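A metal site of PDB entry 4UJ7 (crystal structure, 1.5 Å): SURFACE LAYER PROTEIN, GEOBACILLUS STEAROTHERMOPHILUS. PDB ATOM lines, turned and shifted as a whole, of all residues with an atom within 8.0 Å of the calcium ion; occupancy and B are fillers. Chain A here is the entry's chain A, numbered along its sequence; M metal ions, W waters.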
ATOM      1  N   ILE A 123     -31.483 -22.014  21.319  1.00  0.00           N
ATOM      2  CA  ILE A 123     -31.869 -22.090  19.911  1.00  0.00           C
ATOM      3  C   ILE A 123     -30.857 -21.242  19.142  1.00  0.00           C
ATOM      4  O   ILE A 123     -30.665 -20.059  19.437  1.00  0.00           O
ATOM      5  CB  ILE A 123     -33.289 -21.512  19.686  1.00  0.00           C
ATOM      6  CG1 ILE A 123     -34.354 -22.379  20.382  1.00  0.00           C
ATOM      7  CG2 ILE A 123     -33.574 -21.333  18.195  1.00  0.00           C
ATOM      8  CD1 ILE A 123     -35.694 -21.693  20.572  1.00  0.00           C
ATOM      9  N   ASP A 124     -30.189 -21.860  18.162  1.00  0.00           N
ATOM     10  CA  ASP A 124     -29.114 -21.192  17.427  1.00  0.00           C
ATOM     11  C   ASP A 124     -29.660 -20.684  16.091  1.00  0.00           C
ATOM     12  O   ASP A 124     -29.911 -21.493  15.179  1.00  0.00           O
ATOM     13  CB  ASP A 124     -27.956 -22.179  17.222  1.00  0.00           C
ATOM     14  CG  ASP A 124     -26.683 -21.515  16.700  1.00  0.00           C
ATOM     15  OD1 ASP A 124     -26.735 -20.377  16.190  1.00  0.00           O
ATOM     16  OD2 ASP A 124     -25.625 -22.175  16.811  1.00  0.00           O
ATOM     17  N   LYS A 125     -29.878 -19.376  15.990  1.00  0.00           N
ATOM     18  CA  LYS A 125     -30.471 -18.799  14.774  1.00  0.00           C
ATOM     19  C   LYS A 125     -29.491 -18.667  13.606  1.00  0.00           C
ATOM     20  O   LYS A 125     -29.854 -18.112  12.558  1.00  0.00           O
ATOM     21  CB  LYS A 125     -31.219 -17.491  15.055  1.00  0.00           C
ATOM     22  CG  LYS A 125     -30.362 -16.314  15.494  1.00  0.00           C
ATOM     23  CD  LYS A 125     -31.207 -15.062  15.608  1.00  0.00           C
ATOM     24  CE  LYS A 125     -30.347 -13.831  15.879  1.00  0.00           C
ATOM     25  NZ  LYS A 125     -29.533 -13.447  14.675  1.00  0.00           N
ATOM     26  N   SER A 126     -28.268 -19.158  13.780  1.00  0.00           N
ATOM     27  CA  SER A 126     -27.334 -19.332  12.657  1.00  0.00           C
ATOM     28  C   SER A 126     -27.971 -20.235  11.625  1.00  0.00           C
ATOM     29  O   SER A 126     -28.766 -21.125  11.966  1.00  0.00           O
ATOM     30  CB  SER A 126     -26.025 -19.975  13.134  1.00  0.00           C
ATOM     31  OG  SER A 126     -25.181 -20.332  12.031  1.00  0.00           O
ATOM     32  N   ALA A 127     -27.604 -20.034  10.359  1.00  0.00           N
ATOM     33  CA  ALA A 127     -28.098 -20.862   9.266  1.00  0.00           C
ATOM     34  C   ALA A 127     -27.338 -22.183   9.111  1.00  0.00           C
ATOM     35  O   ALA A 127     -27.819 -23.098   8.456  1.00  0.00           O
ATOM     36  CB  ALA A 127     -28.104 -20.056   7.968  1.00  0.00           C
ATOM     37  N   THR A 128     -26.167 -22.308   9.740  1.00  0.00           N
ATOM     38  CA  THR A 128     -25.292 -23.458   9.439  1.00  0.00           C
ATOM     39  C   THR A 128     -24.645 -24.221  10.612  1.00  0.00           C
ATOM     40  O   THR A 128     -23.699 -24.993  10.373  1.00  0.00           O
ATOM     41  CB  THR A 128     -24.147 -23.052   8.489  1.00  0.00           C
ATOM     42  OG1 THR A 128     -23.590 -21.808   8.925  1.00  0.00           O
ATOM     43  CG2 THR A 128     -24.653 -22.932   7.072  1.00  0.00           C
ATOM     44  N   GLU A 129     -25.109 -24.034  11.836  1.00  0.00           N
ATOM     45  CA  GLU A 129     -24.441 -24.731  12.955  1.00  0.00           C
ATOM     46  C   GLU A 129     -24.525 -26.251  12.798  1.00  0.00           C
ATOM     47  O   GLU A 129     -25.491 -26.786  12.259  1.00  0.00           O
ATOM     48  CB  GLU A 129     -24.928 -24.247  14.335  1.00  0.00           C
ATOM     49  CG  GLU A 129     -26.262 -24.819  14.816  1.00  0.00           C
ATOM     50  CD  GLU A 129     -27.491 -24.194  14.174  1.00  0.00           C
ATOM     51  OE1 GLU A 129     -27.389 -23.228  13.390  1.00  0.00           O
ATOM     52  OE2 GLU A 129     -28.583 -24.699  14.462  1.00  0.00           O
ATOM     53  N   SER A 130     -23.469 -26.950  13.225  1.00  0.00           N
ATOM     54  CA  SER A 130     -23.414 -28.404  13.186  1.00  0.00           C
ATOM     55  C   SER A 130     -22.917 -28.893  14.542  1.00  0.00           C
ATOM     56  O   SER A 130     -21.819 -28.517  14.978  1.00  0.00           O
ATOM     57  CB  SER A 130     -22.474 -28.870  12.065  1.00  0.00           C
ATOM     58  OG  SER A 130     -22.530 -30.273  11.882  1.00  0.00           O
ATOM     59  N   PRO A 131     -23.726 -29.714  15.243  1.00  0.00           N
ATOM     60  CA  PRO A 131     -25.027 -30.243  14.854  1.00  0.00           C
ATOM     61  C   PRO A 131     -26.098 -29.146  14.864  1.00  0.00           C
ATOM     62  O   PRO A 131     -25.929 -28.136  15.536  1.00  0.00           O
ATOM     63  CB  PRO A 131     -25.331 -31.263  15.957  1.00  0.00           C
ATOM     64  CG  PRO A 131     -24.600 -30.771  17.144  1.00  0.00           C
ATOM     65  CD  PRO A 131     -23.378 -30.066  16.636  1.00  0.00           C
ATOM     66  N   ALA A 132     -27.173 -29.347  14.108  1.00  0.00           N
ATOM     67  CA  ALA A 132     -28.295 -28.402  14.120  1.00  0.00           C
ATOM     68  C   ALA A 132     -28.832 -28.237  15.551  1.00  0.00           C
ATOM     69  O   ALA A 132     -28.931 -29.214  16.290  1.00  0.00           O
ATOM     70  CB  ALA A 132     -29.393 -28.869  13.186  1.00  0.00           C
ATOM     71  N   ASN A 133     -29.158 -27.010  15.927  1.00  0.00           N
ATOM     72  CA  ASN A 133     -29.572 -26.714  17.291  1.00  0.00           C
ATOM     73  C   ASN A 133     -30.725 -25.718  17.257  1.00  0.00           C
ATOM     74  O   ASN A 133     -30.592 -24.552  17.646  1.00  0.00           O
ATOM     75  CB  ASN A 133     -28.384 -26.135  18.074  1.00  0.00           C
ATOM     76  CG  ASN A 133     -28.678 -25.942  19.557  1.00  0.00           C
ATOM     77  OD1 ASN A 133     -29.706 -26.408  20.069  1.00  0.00           O
ATOM     78  ND2 ASN A 133     -27.788 -25.229  20.235  1.00  0.00           N
ATOM     79  N   ASN A 134     -31.871 -26.200  16.785  1.00  0.00           N
ATOM     80  CA  ASN A 134     -32.957 -25.289  16.415  1.00  0.00           C
ATOM     81  C   ASN A 134     -34.177 -25.339  17.310  1.00  0.00           C
ATOM     82  O   ASN A 134     -35.233 -24.774  16.993  1.00  0.00           O
ATOM     83  CB  ASN A 134     -33.321 -25.514  14.945  1.00  0.00           C
ATOM     84  CG  ASN A 134     -32.208 -25.068  14.000  1.00  0.00           C
ATOM     85  OD1 ASN A 134     -31.606 -23.998  14.173  1.00  0.00           O
ATOM     86  ND2 ASN A 134     -31.951 -25.893  12.992  1.00  0.00           N
ATOM     87  N   ASP A 135     -34.056 -25.986  18.454  1.00  0.00           N
ATOM     88  CA  ASP A 135     -35.165 -25.988  19.394  1.00  0.00           C
ATOM     89  C   ASP A 135     -34.742 -26.005  20.846  1.00  0.00           C
ATOM     90  O   ASP A 135     -33.546 -26.122  21.168  1.00  0.00           O
ATOM     91  CB  ASP A 135     -36.196 -27.097  19.060  1.00  0.00           C
ATOM     92  CG  ASP A 135     -35.752 -28.517  19.450  1.00  0.00           C
ATOM     93  OD1 ASP A 135     -34.797 -28.708  20.234  1.00  0.00           O
ATOM     94  OD2 ASP A 135     -36.424 -29.461  18.996  1.00  0.00           O
ATOM     95  N   ASP A 188     -37.482 -20.895  16.975  1.00  0.00           N
ATOM     96  CA  ASP A 188     -37.354 -19.489  16.548  1.00  0.00           C
ATOM     97  C   ASP A 188     -38.543 -19.120  15.670  1.00  0.00           C
ATOM     98  O   ASP A 188     -39.025 -19.924  14.866  1.00  0.00           O
ATOM     99  CB  ASP A 188     -36.062 -19.319  15.754  1.00  0.00           C
ATOM    100  CG  ASP A 188     -35.729 -17.871  15.430  1.00  0.00           C
ATOM    101  OD1 ASP A 188     -36.246 -16.965  16.094  1.00  0.00           O
ATOM    102  OD2 ASP A 188     -34.868 -17.660  14.534  1.00  0.00           O
ATOM    103  N   ILE A 216     -29.253 -17.882  20.549  1.00  0.00           N
ATOM    104  CA  ILE A 216     -27.839 -17.580  20.271  1.00  0.00           C
ATOM    105  C   ILE A 216     -27.650 -17.524  18.745  1.00  0.00           C
ATOM    106  O   ILE A 216     -28.557 -17.875  17.969  1.00  0.00           O
ATOM    107  CB  ILE A 216     -26.881 -18.632  20.924  1.00  0.00           C
ATOM    108  CG1 ILE A 216     -27.061 -20.021  20.277  1.00  0.00           C
ATOM    109  CG2 ILE A 216     -27.061 -18.650  22.434  1.00  0.00           C
ATOM    110  CD1 ILE A 216     -26.013 -21.075  20.674  1.00  0.00           C
ATOM    111  N   ASP A 217     -26.482 -17.073  18.293  1.00  0.00           N
ATOM    112  CA  ASP A 217     -26.161 -17.125  16.882  1.00  0.00           C
ATOM    113  C   ASP A 217     -24.666 -17.366  16.735  1.00  0.00           C
ATOM    114  O   ASP A 217     -23.862 -16.460  16.967  1.00  0.00           O
ATOM    115  CB  ASP A 217     -26.548 -15.806  16.189  1.00  0.00           C
ATOM    116  CG  ASP A 217     -26.474 -15.890  14.660  1.00  0.00           C
ATOM    117  OD1 ASP A 217     -25.637 -16.658  14.126  1.00  0.00           O
ATOM    118  OD2 ASP A 217     -27.259 -15.177  13.982  1.00  0.00           O
ATOM    119  N   THR A 218     -24.297 -18.583  16.333  1.00  0.00           N
ATOM    120  CA  THR A 218     -22.869 -18.959  16.296  1.00  0.00           C
ATOM    121  C   THR A 218     -22.242 -18.769  14.921  1.00  0.00           C
ATOM    122  O   THR A 218     -21.129 -19.248  14.706  1.00  0.00           O
ATOM    123  CB  THR A 218     -22.643 -20.414  16.763  1.00  0.00           C
ATOM    124  OG1 THR A 218     -23.344 -21.314  15.891  1.00  0.00           O
ATOM    125  CG2 THR A 218     -23.098 -20.601  18.221  1.00  0.00           C
ATOM    126  N   THR A 219     -22.930 -18.066  14.009  1.00  0.00           N
ATOM    127  CA  THR A 219     -22.395 -17.812  12.663  1.00  0.00           C
ATOM    128  C   THR A 219     -20.994 -17.191  12.764  1.00  0.00           C
ATOM    129  O   THR A 219     -20.709 -16.342  13.622  1.00  0.00           O
ATOM    130  CB  THR A 219     -23.302 -16.884  11.834  1.00  0.00           C
ATOM    131  OG1 THR A 219     -24.631 -17.419  11.788  1.00  0.00           O
ATOM    132  CG2 THR A 219     -22.777 -16.749  10.401  1.00  0.00           C
ATOM    133  OXT THR A 219     -20.118 -17.547  11.982  1.00  0.00           O
HETATM  134 CA    CA M   1     -29.739 -22.881  13.264  1.00  0.00          CA
HETATM  135  O   HOH W   1     -29.805 -24.338  11.352  1.00  0.00           O
HETATM  136  O   HOH W   2     -31.648 -21.993  12.105  1.00  0.00           O
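The side-chain amide oxygen (OD1) of Asn 134 binds the calcium ion. O of Asp 124 is bound to the calcium ion (2.4 Å). The calcium ion is bound by the side-chain carboxylate (OE1) of Glu 129 (2.4 Å). The calcium ion is bound by the backbone carbonyl oxygen (O) of Ser 126. Water W2 is bound to the calcium ion, 2.4 Å away. The calcium ion is bound by water W1, 2.4 Å away. OE2 of Glu 129 is bound to the calcium ion (2.5 Å).
Four residues have an atom within 4 Å of the calcium ion: Asp 124, Ser 126, Glu 129 and Asn 134. The nearest printed residue that does not touch the calcium ion is Lys 125 (4.2 Å).
N of Ser 126 lies close to OD1 of Asp 124 (3.1 Å). The side-chain hydroxyl (OG1) of Thr 219 is in hydrogen-bond range of the side-chain hydroxyl (OG) of Ser 126 (3.0 Å). The backbone carbonyl oxygen of Asn 133 is in hydrogen-bond range of the backbone NH of Asp 124 (2.8 Å). The side-chain carboxylate (OD2) of Asp 124 is in hydrogen-bond range of the side-chain hydroxyl (OG1) of Thr 218 (2.6 Å). OE2 of Glu 129 sits close to N of Asn 133 (2.8 Å). The side-chain hydroxyl (OG) of Ser 126 lies within hydrogen-bond range of the backbone NH (N) of Thr 128 (3.2 Å).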
